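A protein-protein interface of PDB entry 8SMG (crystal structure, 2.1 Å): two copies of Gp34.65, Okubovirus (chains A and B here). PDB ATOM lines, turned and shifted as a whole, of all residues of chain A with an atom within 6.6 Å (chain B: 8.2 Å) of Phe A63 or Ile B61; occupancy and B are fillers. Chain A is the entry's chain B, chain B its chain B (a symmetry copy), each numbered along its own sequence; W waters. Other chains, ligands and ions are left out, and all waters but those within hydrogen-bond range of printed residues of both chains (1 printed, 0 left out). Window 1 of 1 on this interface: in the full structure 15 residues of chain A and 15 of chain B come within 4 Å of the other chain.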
ATOM      1  N   LEU A  15     -31.545  11.424   2.623  1.00  0.00           N
ATOM      2  CA  LEU A  15     -31.521  11.494   4.081  1.00  0.00           C
ATOM      3  C   LEU A  15     -31.629  12.934   4.565  1.00  0.00           C
ATOM      4  O   LEU A  15     -32.381  13.227   5.501  1.00  0.00           O
ATOM      5  CB  LEU A  15     -30.247  10.842   4.620  1.00  0.00           C
ATOM      6  CG  LEU A  15     -30.194   9.313   4.606  1.00  0.00           C
ATOM      7  CD1 LEU A  15     -28.818   8.820   5.024  1.00  0.00           C
ATOM      8  CD2 LEU A  15     -31.270   8.740   5.512  1.00  0.00           C
ATOM      9  N   PHE A  32     -32.984   0.358   7.942  1.00  0.00           N
ATOM     10  CA  PHE A  32     -32.982   1.613   7.204  1.00  0.00           C
ATOM     11  C   PHE A  32     -32.290   2.691   8.026  1.00  0.00           C
ATOM     12  O   PHE A  32     -32.101   2.553   9.238  1.00  0.00           O
ATOM     13  CB  PHE A  32     -34.404   2.054   6.828  1.00  0.00           C
ATOM     14  CG  PHE A  32     -35.318   2.254   8.009  1.00  0.00           C
ATOM     15  CD1 PHE A  32     -35.356   3.467   8.679  1.00  0.00           C
ATOM     16  CD2 PHE A  32     -36.153   1.233   8.435  1.00  0.00           C
ATOM     17  CE1 PHE A  32     -36.199   3.655   9.762  1.00  0.00           C
ATOM     18  CE2 PHE A  32     -36.998   1.415   9.516  1.00  0.00           C
ATOM     19  CZ  PHE A  32     -37.022   2.627  10.180  1.00  0.00           C
ATOM     20  N   LEU A  33     -31.928   3.775   7.344  1.00  0.00           N
ATOM     21  CA  LEU A  33     -31.293   4.929   7.959  1.00  0.00           C
ATOM     22  C   LEU A  33     -32.244   6.119   7.950  1.00  0.00           C
ATOM     23  O   LEU A  33     -33.126   6.221   7.093  1.00  0.00           O
ATOM     24  CB  LEU A  33     -30.006   5.311   7.222  1.00  0.00           C
ATOM     25  CG  LEU A  33     -29.030   4.199   6.839  1.00  0.00           C
ATOM     26  CD1 LEU A  33     -27.912   4.768   5.987  1.00  0.00           C
ATOM     27  CD2 LEU A  33     -28.468   3.525   8.076  1.00  0.00           C
ATOM     28  N   PHE A  34     -32.052   7.024   8.908  1.00  0.00           N
ATOM     29  CA  PHE A  34     -32.786   8.281   8.923  1.00  0.00           C
ATOM     30  C   PHE A  34     -31.952   9.328   9.646  1.00  0.00           C
ATOM     31  O   PHE A  34     -31.265   9.021  10.624  1.00  0.00           O
ATOM     32  CB  PHE A  34     -34.169   8.136   9.577  1.00  0.00           C
ATOM     33  CG  PHE A  34     -34.130   7.699  11.016  1.00  0.00           C
ATOM     34  CD1 PHE A  34     -34.115   6.353  11.344  1.00  0.00           C
ATOM     35  CD2 PHE A  34     -34.134   8.634  12.039  1.00  0.00           C
ATOM     36  CE1 PHE A  34     -34.089   5.947  12.666  1.00  0.00           C
ATOM     37  CE2 PHE A  34     -34.105   8.236  13.364  1.00  0.00           C
ATOM     38  CZ  PHE A  34     -34.085   6.891  13.677  1.00  0.00           C
ATOM     39  N   LEU A  35     -32.014  10.562   9.149  1.00  0.00           N
ATOM     40  CA  LEU A  35     -31.210  11.664   9.659  1.00  0.00           C
ATOM     41  C   LEU A  35     -32.074  12.590  10.503  1.00  0.00           C
ATOM     42  O   LEU A  35     -33.144  13.021  10.061  1.00  0.00           O
ATOM     43  CB  LEU A  35     -30.573  12.442   8.506  1.00  0.00           C
ATOM     44  CG  LEU A  35     -29.726  13.667   8.861  1.00  0.00           C
ATOM     45  CD1 LEU A  35     -28.400  13.246   9.456  1.00  0.00           C
ATOM     46  CD2 LEU A  35     -29.507  14.546   7.642  1.00  0.00           C
ATOM     47  N   LYS A  36     -31.611  12.891  11.713  1.00  0.00           N
ATOM     48  CA  LYS A  36     -32.274  13.830  12.606  1.00  0.00           C
ATOM     49  C   LYS A  36     -31.464  15.117  12.671  1.00  0.00           C
ATOM     50  O   LYS A  36     -30.244  15.079  12.870  1.00  0.00           O
ATOM     51  CB  LYS A  36     -32.442  13.238  14.007  1.00  0.00           C
ATOM     52  CG  LYS A  36     -33.403  12.061  14.078  1.00  0.00           C
ATOM     53  CD  LYS A  36     -34.841  12.498  13.846  1.00  0.00           C
ATOM     54  CE  LYS A  36     -35.332  13.398  14.967  1.00  0.00           C
ATOM     55  NZ  LYS A  36     -36.757  13.787  14.779  1.00  0.00           N
ATOM     56  N   LEU A  41     -32.755  17.355  17.589  1.00  0.00           N
ATOM     57  CA  LEU A  41     -31.977  16.585  18.552  1.00  0.00           C
ATOM     58  C   LEU A  41     -31.987  17.230  19.933  1.00  0.00           C
ATOM     59  O   LEU A  41     -32.009  16.524  20.948  1.00  0.00           O
ATOM     60  CB  LEU A  41     -30.542  16.421  18.052  1.00  0.00           C
ATOM     61  CG  LEU A  41     -30.346  15.413  16.920  1.00  0.00           C
ATOM     62  CD1 LEU A  41     -29.024  15.659  16.228  1.00  0.00           C
ATOM     63  CD2 LEU A  41     -30.417  13.992  17.452  1.00  0.00           C
ATOM     64  N   ILE A  61     -27.296  13.914  12.749  1.00  0.00           N
ATOM     65  CA  ILE A  61     -26.926  12.568  13.172  1.00  0.00           C
ATOM     66  C   ILE A  61     -27.699  11.558  12.338  1.00  0.00           C
ATOM     67  O   ILE A  61     -28.930  11.628  12.250  1.00  0.00           O
ATOM     68  CB  ILE A  61     -27.194  12.342  14.673  1.00  0.00           C
ATOM     69  CG1 ILE A  61     -26.342  13.291  15.518  1.00  0.00           C
ATOM     70  CG2 ILE A  61     -26.912  10.895  15.045  1.00  0.00           C
ATOM     71  CD1 ILE A  61     -26.509  13.094  17.008  1.00  0.00           C
ATOM     72  N   ILE A  62     -26.979  10.616  11.736  1.00  0.00           N
ATOM     73  CA  ILE A  62     -27.588   9.521  10.992  1.00  0.00           C
ATOM     74  C   ILE A  62     -27.787   8.343  11.935  1.00  0.00           C
ATOM     75  O   ILE A  62     -26.834   7.876  12.572  1.00  0.00           O
ATOM     76  CB  ILE A  62     -26.721   9.117   9.790  1.00  0.00           C
ATOM     77  CG1 ILE A  62     -26.360  10.340   8.946  1.00  0.00           C
ATOM     78  CG2 ILE A  62     -27.442   8.074   8.944  1.00  0.00           C
ATOM     79  CD1 ILE A  62     -25.451  10.025   7.777  1.00  0.00           C
ATOM     80  N   PHE A  63     -29.021   7.862  12.023  1.00  0.00           N
ATOM     81  CA  PHE A  63     -29.370   6.710  12.839  1.00  0.00           C
ATOM     82  C   PHE A  63     -29.632   5.501  11.950  1.00  0.00           C
ATOM     83  O   PHE A  63     -29.784   5.613  10.730  1.00  0.00           O
ATOM     84  CB  PHE A  63     -30.601   7.008  13.704  1.00  0.00           C
ATOM     85  CG  PHE A  63     -30.393   8.119  14.688  1.00  0.00           C
ATOM     86  CD1 PHE A  63     -29.858   7.860  15.938  1.00  0.00           C
ATOM     87  CD2 PHE A  63     -30.730   9.422  14.363  1.00  0.00           C
ATOM     88  CE1 PHE A  63     -29.664   8.882  16.847  1.00  0.00           C
ATOM     89  CE2 PHE A  63     -30.538  10.448  15.269  1.00  0.00           C
ATOM     90  CZ  PHE A  63     -30.006  10.177  16.513  1.00  0.00           C
ATOM     91  N   ILE A  64     -29.688   4.332  12.583  1.00  0.00           N
ATOM     92  CA  ILE A  64     -29.974   3.080  11.893  1.00  0.00           C
ATOM     93  C   ILE A  64     -30.963   2.275  12.724  1.00  0.00           C
ATOM     94  O   ILE A  64     -30.740   2.047  13.917  1.00  0.00           O
ATOM     95  CB  ILE A  64     -28.694   2.258  11.632  1.00  0.00           C
ATOM     96  CG1 ILE A  64     -29.045   0.810  11.279  1.00  0.00           C
ATOM     97  CG2 ILE A  64     -27.771   2.297  12.837  1.00  0.00           C
ATOM     98  CD1 ILE A  64     -29.636   0.634   9.902  1.00  0.00           C
ATOM     99  N   LYS A  65     -32.060   1.856  12.097  1.00  0.00           N
ATOM    100  CA  LYS A  65     -32.970   0.881  12.688  1.00  0.00           C
ATOM    101  C   LYS A  65     -32.429  -0.506  12.356  1.00  0.00           C
ATOM    102  O   LYS A  65     -32.465  -0.932  11.196  1.00  0.00           O
ATOM    103  CB  LYS A  65     -34.391   1.074  12.164  1.00  0.00           C
ATOM    104  CG  LYS A  65     -35.421   0.103  12.743  1.00  0.00           C
ATOM    105  CD  LYS A  65     -35.633  -1.096  11.827  1.00  0.00           C
ATOM    106  CE  LYS A  65     -36.463  -2.173  12.499  1.00  0.00           C
ATOM    107  NZ  LYS A  65     -36.516  -3.414  11.679  1.00  0.00           N
ATOM    108  N   ILE A  71     -32.512   1.166  17.682  1.00  0.00           N
ATOM    109  CA  ILE A  71     -32.085   2.416  17.063  1.00  0.00           C
ATOM    110  C   ILE A  71     -30.700   2.755  17.599  1.00  0.00           C
ATOM    111  O   ILE A  71     -30.535   3.026  18.794  1.00  0.00           O
ATOM    112  CB  ILE A  71     -33.079   3.554  17.330  1.00  0.00           C
ATOM    113  CG1 ILE A  71     -34.445   3.218  16.724  1.00  0.00           C
ATOM    114  CG2 ILE A  71     -32.552   4.864  16.767  1.00  0.00           C
ATOM    115  CD1 ILE A  71     -35.483   4.304  16.911  1.00  0.00           C
ATOM    116  N   HIS A  72     -29.707   2.739  16.714  1.00  0.00           N
ATOM    117  CA  HIS A  72     -28.330   3.066  17.046  1.00  0.00           C
ATOM    118  C   HIS A  72     -27.838   4.203  16.160  1.00  0.00           C
ATOM    119  O   HIS A  72     -28.425   4.505  15.118  1.00  0.00           O
ATOM    120  CB  HIS A  72     -27.401   1.853  16.864  1.00  0.00           C
ATOM    121  CG  HIS A  72     -27.639   0.747  17.843  1.00  0.00           C
ATOM    122  ND1 HIS A  72     -26.747   0.440  18.849  1.00  0.00           N
ATOM    123  CD2 HIS A  72     -28.661  -0.134  17.965  1.00  0.00           C
ATOM    124  CE1 HIS A  72     -27.212  -0.578  19.551  1.00  0.00           C
ATOM    125  NE2 HIS A  72     -28.371  -0.945  19.036  1.00  0.00           N
ATOM    126  N   ALA A  73     -26.746   4.832  16.585  1.00  0.00           N
ATOM    127  CA  ALA A  73     -26.026   5.737  15.702  1.00  0.00           C
ATOM    128  C   ALA A  73     -25.338   4.923  14.614  1.00  0.00           C
ATOM    129  O   ALA A  73     -24.708   3.899  14.900  1.00  0.00           O
ATOM    130  CB  ALA A  73     -25.004   6.554  16.489  1.00  0.00           C
ATOM    131  N   TRP A  74     -25.471   5.363  13.364  1.00  0.00           N
ATOM    132  CA  TRP A  74     -24.995   4.571  12.238  1.00  0.00           C
ATOM    133  C   TRP A  74     -23.517   4.818  11.977  1.00  0.00           C
ATOM    134  O   TRP A  74     -23.031   5.949  12.059  1.00  0.00           O
ATOM    135  CB  TRP A  74     -25.802   4.875  10.974  1.00  0.00           C
ATOM    136  CG  TRP A  74     -25.388   4.033   9.790  1.00  0.00           C
ATOM    137  CD1 TRP A  74     -25.377   2.672   9.719  1.00  0.00           C
ATOM    138  CD2 TRP A  74     -24.940   4.505   8.510  1.00  0.00           C
ATOM    139  NE1 TRP A  74     -24.943   2.267   8.479  1.00  0.00           N
ATOM    140  CE2 TRP A  74     -24.670   3.372   7.718  1.00  0.00           C
ATOM    141  CE3 TRP A  74     -24.739   5.775   7.960  1.00  0.00           C
ATOM    142  CZ2 TRP A  74     -24.212   3.468   6.406  1.00  0.00           C
ATOM    143  CZ3 TRP A  74     -24.283   5.870   6.657  1.00  0.00           C
ATOM    144  CH2 TRP A  74     -24.024   4.722   5.894  1.00  0.00           C
ATOM    145  N   LEU B  15     -17.049   4.964  29.787  1.00  0.00           N
ATOM    146  CA  LEU B  15     -18.183   5.547  29.076  1.00  0.00           C
ATOM    147  C   LEU B  15     -19.498   4.945  29.552  1.00  0.00           C
ATOM    148  O   LEU B  15     -20.473   5.670  29.780  1.00  0.00           O
ATOM    149  CB  LEU B  15     -18.017   5.353  27.568  1.00  0.00           C
ATOM    150  CG  LEU B  15     -17.002   6.252  26.863  1.00  0.00           C
ATOM    151  CD1 LEU B  15     -16.841   5.840  25.408  1.00  0.00           C
ATOM    152  CD2 LEU B  15     -17.424   7.707  26.967  1.00  0.00           C
ATOM    153  N   LEU B  33     -15.621  11.999  24.362  1.00  0.00           N
ATOM    154  CA  LEU B  33     -16.765  11.144  24.090  1.00  0.00           C
ATOM    155  C   LEU B  33     -17.642  11.030  25.331  1.00  0.00           C
ATOM    156  O   LEU B  33     -17.166  11.167  26.460  1.00  0.00           O
ATOM    157  CB  LEU B  33     -16.322   9.743  23.661  1.00  0.00           C
ATOM    158  CG  LEU B  33     -15.199   9.619  22.630  1.00  0.00           C
ATOM    159  CD1 LEU B  33     -14.811   8.162  22.467  1.00  0.00           C
ATOM    160  CD2 LEU B  33     -15.621  10.211  21.300  1.00  0.00           C
ATOM    161  N   PHE B  34     -18.930  10.770  25.111  1.00  0.00           N
ATOM    162  CA  PHE B  34     -19.844  10.483  26.206  1.00  0.00           C
ATOM    163  C   PHE B  34     -20.978   9.613  25.686  1.00  0.00           C
ATOM    164  O   PHE B  34     -21.433   9.784  24.552  1.00  0.00           O
ATOM    165  CB  PHE B  34     -20.392  11.766  26.854  1.00  0.00           C
ATOM    166  CG  PHE B  34     -21.179  12.643  25.919  1.00  0.00           C
ATOM    167  CD1 PHE B  34     -20.543  13.606  25.151  1.00  0.00           C
ATOM    168  CD2 PHE B  34     -22.557  12.521  25.826  1.00  0.00           C
ATOM    169  CE1 PHE B  34     -21.263  14.421  24.297  1.00  0.00           C
ATOM    170  CE2 PHE B  34     -23.284  13.331  24.973  1.00  0.00           C
ATOM    171  CZ  PHE B  34     -22.637  14.283  24.208  1.00  0.00           C
ATOM    172  N   LEU B  35     -21.420   8.676  26.521  1.00  0.00           N
ATOM    173  CA  LEU B  35     -22.432   7.697  26.152  1.00  0.00           C
ATOM    174  C   LEU B  35     -23.766   8.065  26.789  1.00  0.00           C
ATOM    175  O   LEU B  35     -23.837   8.305  27.999  1.00  0.00           O
ATOM    176  CB  LEU B  35     -22.009   6.294  26.591  1.00  0.00           C
ATOM    177  CG  LEU B  35     -22.981   5.144  26.321  1.00  0.00           C
ATOM    178  CD1 LEU B  35     -23.005   4.798  24.848  1.00  0.00           C
ATOM    179  CD2 LEU B  35     -22.621   3.923  27.149  1.00  0.00           C
ATOM    180  N   LYS B  36     -24.817   8.111  25.975  1.00  0.00           N
ATOM    181  CA  LYS B  36     -26.174   8.360  26.443  1.00  0.00           C
ATOM    182  C   LYS B  36     -26.973   7.067  26.370  1.00  0.00           C
ATOM    183  O   LYS B  36     -26.962   6.381  25.342  1.00  0.00           O
ATOM    184  CB  LYS B  36     -26.853   9.452  25.612  1.00  0.00           C
ATOM    185  CG  LYS B  36     -26.243  10.835  25.779  1.00  0.00           C
ATOM    186  CD  LYS B  36     -26.514  11.404  27.161  1.00  0.00           C
ATOM    187  CE  LYS B  36     -27.996  11.666  27.369  1.00  0.00           C
ATOM    188  NZ  LYS B  36     -28.268  12.276  28.700  1.00  0.00           N
ATOM    189  N   SER B  37     -27.665   6.742  27.460  1.00  0.00           N
ATOM    190  CA  SER B  37     -28.414   5.499  27.551  1.00  0.00           C
ATOM    191  C   SER B  37     -29.715   5.587  26.760  1.00  0.00           C
ATOM    192  O   SER B  37     -30.185   6.668  26.397  1.00  0.00           O
ATOM    193  CB  SER B  37     -28.714   5.156  29.011  1.00  0.00           C
ATOM    194  OG  SER B  37     -29.464   3.958  29.113  1.00  0.00           O
ATOM    195  N   SER B  38     -30.301   4.414  26.502  1.00  0.00           N
ATOM    196  CA  SER B  38     -31.534   4.347  25.724  1.00  0.00           C
ATOM    197  C   SER B  38     -32.669   5.091  26.417  1.00  0.00           C
ATOM    198  O   SER B  38     -33.483   5.752  25.758  1.00  0.00           O
ATOM    199  CB  SER B  38     -31.920   2.888  25.487  1.00  0.00           C
ATOM    200  OG  SER B  38     -32.137   2.211  26.713  1.00  0.00           O
ATOM    201  N   LEU B  41     -32.261   8.703  25.885  1.00  0.00           N
ATOM    202  CA  LEU B  41     -32.391   9.092  24.485  1.00  0.00           C
ATOM    203  C   LEU B  41     -33.848   9.311  24.093  1.00  0.00           C
ATOM    204  O   LEU B  41     -34.148  10.206  23.295  1.00  0.00           O
ATOM    205  CB  LEU B  41     -31.751   8.034  23.588  1.00  0.00           C
ATOM    206  CG  LEU B  41     -30.223   8.027  23.558  1.00  0.00           C
ATOM    207  CD1 LEU B  41     -29.720   6.706  23.021  1.00  0.00           C
ATOM    208  CD2 LEU B  41     -29.700   9.181  22.722  1.00  0.00           C
ATOM    209  N   PHE B  58     -34.544   2.565  21.617  1.00  0.00           N
ATOM    210  CA  PHE B  58     -33.200   3.086  21.441  1.00  0.00           C
ATOM    211  C   PHE B  58     -32.166   2.114  22.005  1.00  0.00           C
ATOM    212  O   PHE B  58     -32.458   1.262  22.849  1.00  0.00           O
ATOM    213  CB  PHE B  58     -33.052   4.447  22.127  1.00  0.00           C
ATOM    214  CG  PHE B  58     -33.282   5.621  21.215  1.00  0.00           C
ATOM    215  CD1 PHE B  58     -32.268   6.084  20.393  1.00  0.00           C
ATOM    216  CD2 PHE B  58     -34.505   6.273  21.195  1.00  0.00           C
ATOM    217  CE1 PHE B  58     -32.472   7.166  19.558  1.00  0.00           C
ATOM    218  CE2 PHE B  58     -34.714   7.356  20.362  1.00  0.00           C
ATOM    219  CZ  PHE B  58     -33.695   7.803  19.543  1.00  0.00           C
ATOM    220  N   GLY B  59     -30.938   2.242  21.499  1.00  0.00           N
ATOM    221  CA  GLY B  59     -29.787   1.602  22.091  1.00  0.00           C
ATOM    222  C   GLY B  59     -28.789   2.667  22.517  1.00  0.00           C
ATOM    223  O   GLY B  59     -28.913   3.838  22.153  1.00  0.00           O
ATOM    224  N   ASN B  60     -27.800   2.249  23.306  1.00  0.00           N
ATOM    225  CA  ASN B  60     -26.773   3.180  23.759  1.00  0.00           C
ATOM    226  C   ASN B  60     -26.067   3.819  22.568  1.00  0.00           C
ATOM    227  O   ASN B  60     -25.794   3.161  21.562  1.00  0.00           O
ATOM    228  CB  ASN B  60     -25.760   2.458  24.649  1.00  0.00           C
ATOM    229  CG  ASN B  60     -26.356   2.016  25.971  1.00  0.00           C
ATOM    230  OD1 ASN B  60     -26.433   2.794  26.921  1.00  0.00           O
ATOM    231  ND2 ASN B  60     -26.775   0.758  26.040  1.00  0.00           N
ATOM    232  N   ILE B  61     -25.784   5.116  22.684  1.00  0.00           N
ATOM    233  CA  ILE B  61     -25.179   5.887  21.604  1.00  0.00           C
ATOM    234  C   ILE B  61     -23.980   6.647  22.150  1.00  0.00           C
ATOM    235  O   ILE B  61     -24.096   7.370  23.146  1.00  0.00           O
ATOM    236  CB  ILE B  61     -26.184   6.862  20.961  1.00  0.00           C
ATOM    237  CG1 ILE B  61     -27.343   6.095  20.321  1.00  0.00           C
ATOM    238  CG2 ILE B  61     -25.484   7.732  19.928  1.00  0.00           C
ATOM    239  CD1 ILE B  61     -28.348   6.983  19.622  1.00  0.00           C
ATOM    240  N   ILE B  62     -22.834   6.490  21.495  1.00  0.00           N
ATOM    241  CA  ILE B  62     -21.628   7.234  21.838  1.00  0.00           C
ATOM    242  C   ILE B  62     -21.586   8.504  20.999  1.00  0.00           C
ATOM    243  O   ILE B  62     -21.652   8.448  19.766  1.00  0.00           O
ATOM    244  CB  ILE B  62     -20.368   6.385  21.607  1.00  0.00           C
ATOM    245  CG1 ILE B  62     -20.497   5.025  22.294  1.00  0.00           C
ATOM    246  CG2 ILE B  62     -19.133   7.124  22.106  1.00  0.00           C
ATOM    247  CD1 ILE B  62     -19.316   4.109  22.055  1.00  0.00           C
ATOM    248  N   PHE B  63     -21.474   9.645  21.667  1.00  0.00           N
ATOM    249  CA  PHE B  63     -21.369  10.941  21.017  1.00  0.00           C
ATOM    250  C   PHE B  63     -19.942  11.464  21.120  1.00  0.00           C
ATOM    251  O   PHE B  63     -19.121  10.958  21.889  1.00  0.00           O
ATOM    252  CB  PHE B  63     -22.347  11.944  21.640  1.00  0.00           C
ATOM    253  CG  PHE B  63     -23.787  11.559  21.487  1.00  0.00           C
ATOM    254  CD1 PHE B  63     -24.495  11.919  20.352  1.00  0.00           C
ATOM    255  CD2 PHE B  63     -24.433  10.835  22.474  1.00  0.00           C
ATOM    256  CE1 PHE B  63     -25.823  11.565  20.206  1.00  0.00           C
ATOM    257  CE2 PHE B  63     -25.761  10.477  22.332  1.00  0.00           C
ATOM    258  CZ  PHE B  63     -26.457  10.845  21.198  1.00  0.00           C
ATOM    259  N   ILE B  64     -19.658  12.499  20.335  1.00  0.00           N
ATOM    260  CA  ILE B  64     -18.353  13.152  20.338  1.00  0.00           C
ATOM    261  C   ILE B  64     -18.559  14.659  20.312  1.00  0.00           C
ATOM    262  O   ILE B  64     -19.277  15.181  19.452  1.00  0.00           O
ATOM    263  CB  ILE B  64     -17.479  12.705  19.147  1.00  0.00           C
ATOM    264  CG1 ILE B  64     -16.306  13.669  18.947  1.00  0.00           C
ATOM    265  CG2 ILE B  64     -18.304  12.608  17.876  1.00  0.00           C
ATOM    266  CD1 ILE B  64     -15.227  13.557  19.994  1.00  0.00           C
ATOM    267  N   HIS B  72     -21.708  15.311  17.598  1.00  0.00           N
ATOM    268  CA  HIS B  72     -22.018  14.355  16.546  1.00  0.00           C
ATOM    269  C   HIS B  72     -22.044  12.944  17.119  1.00  0.00           C
ATOM    270  O   HIS B  72     -21.528  12.683  18.208  1.00  0.00           O
ATOM    271  CB  HIS B  72     -20.987  14.414  15.408  1.00  0.00           C
ATOM    272  CG  HIS B  72     -21.022  15.681  14.612  1.00  0.00           C
ATOM    273  ND1 HIS B  72     -21.475  15.729  13.311  1.00  0.00           N
ATOM    274  CD2 HIS B  72     -20.650  16.945  14.928  1.00  0.00           C
ATOM    275  CE1 HIS B  72     -21.386  16.969  12.862  1.00  0.00           C
ATOM    276  NE2 HIS B  72     -20.889  17.726  13.823  1.00  0.00           N
ATOM    277  N   ALA B  73     -22.654  12.030  16.369  1.00  0.00           N
ATOM    278  CA  ALA B  73     -22.505  10.613  16.665  1.00  0.00           C
ATOM    279  C   ALA B  73     -21.082  10.185  16.332  1.00  0.00           C
ATOM    280  O   ALA B  73     -20.557  10.528  15.268  1.00  0.00           O
ATOM    281  CB  ALA B  73     -23.515   9.790  15.871  1.00  0.00           C
ATOM    282  N   TRP B  74     -20.450   9.452  17.245  1.00  0.00           N
ATOM    283  CA  TRP B  74     -19.036   9.131  17.098  1.00  0.00           C
ATOM    284  C   TRP B  74     -18.839   7.896  16.231  1.00  0.00           C
ATOM    285  O   TRP B  74     -19.585   6.921  16.324  1.00  0.00           O
ATOM    286  CB  TRP B  74     -18.378   8.914  18.463  1.00  0.00           C
ATOM    287  CG  TRP B  74     -16.896   8.640  18.369  1.00  0.00           C
ATOM    288  CD1 TRP B  74     -15.951   9.437  17.796  1.00  0.00           C
ATOM    289  CD2 TRP B  74     -16.197   7.493  18.877  1.00  0.00           C
ATOM    290  NE1 TRP B  74     -14.710   8.858  17.908  1.00  0.00           N
ATOM    291  CE2 TRP B  74     -14.834   7.664  18.568  1.00  0.00           C
ATOM    292  CE3 TRP B  74     -16.595   6.337  19.559  1.00  0.00           C
ATOM    293  CZ2 TRP B  74     -13.865   6.726  18.917  1.00  0.00           C
ATOM    294  CZ3 TRP B  74     -15.630   5.407  19.906  1.00  0.00           C
ATOM    295  CH2 TRP B  74     -14.279   5.607  19.584  1.00  0.00           C
HETATM  296  O   HOH W   1     -25.508   3.496  19.153  1.00  0.00           O
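Hydrophobic or aromatic side chains of chain A that line the printed part of chain B: Ile A61, Phe A63, Ile A71, His A72 and Ala A73.
Of the 18 printed residues of chain B, 6 touch a printed residue of chain A.
Hydrophobic or aromatic side chains of chain B within 4 Å of the printed part of chain A: Phe B58, Ile B61, Phe B63 and Ala B73.
Among the printed residues, no Asp or Glu carboxylate lies within 4 Å of a Lys or Arg side-chain nitrogen of the other chain.
Water W1 lies within hydrogen-bond range of the backbone carbonyl oxygen of Asn B60 (2.4 Å), the backbone NH of Ala A73 (3.1 Å) and a ring nitrogen (ND1) of His A72 (3.3 Å).
N of Lys B36 lies within hydrogen-bond range of O of Ile B61, at 3.0 Å.
The backbone carbonyl oxygen of His A72 is in hydrogen-bond range of the backbone NH of Ile A64 (2.8 Å).
The backbone carbonyl oxygen (O) of Phe A34 lies within hydrogen-bond range of the backbone NH (N) of Phe A63, 2.9 Å away.
The backbone carbonyl oxygen of Phe B34 is in hydrogen-bond range of the backbone NH of Phe B63 (2.9 Å).
The backbone NH (N) of Lys A36 is in hydrogen-bond range of the backbone carbonyl oxygen (O) of Ile A61 (3.0 Å).
The backbone carbonyl oxygen of Ile A71 is in hydrogen-bond range of the backbone NH of Gly B59 (2.8 Å).
Phe A63 touches one residue of chain B.
Of the printed residues of chain A, Ile B61 touches Phe A63 (3.6 Å) and Ala A73 (3.7 Å).
Of the printed residues of chain A, Ala B73 touches Ile A61 and Ala A73.
Printed residues of chain B within 4 Å of Ile A71: Phe B58 and Gly B59.
Of the printed residues of chain B, Ala A73 touches Ile B61 and Ala B73.
Printed residues of chain A within 4 Å of Phe B63: Ile A61.
The nearest residue of chain B that does not touch Phe A63 is Phe B58 (4.3 Å).
The nearest printed residue of chain B that does not touch Ile A61 is His B72 (4.5 Å).
Ile A61 touches Phe B63.
Ala B73 touches Ile A61 (CB to CG2, 3.7 Å).
CE1 of Phe A63 touches CD1 of Ile B61, at 3.6 Å.
Ile A71 touches Phe B58 (CG2 to CE1, 3.6 Å).
His A72 touches Asn B60 (ND1 to O, 3.96 Å).
Ala A73 touches Ile B61 (CB to CG2, 3.7 Å).
CB of Ala A73 touches CB of Ala B73, 3.6 Å away.
Ile A61 touches Phe B63, and with the chains exchanged Phe A63 touches Ile B61.
Ile A61 touches Ala B73, and with the chains exchanged Ala A73 touches Ile B61.
Ala A73 touches its own counterpart, Ala B73.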
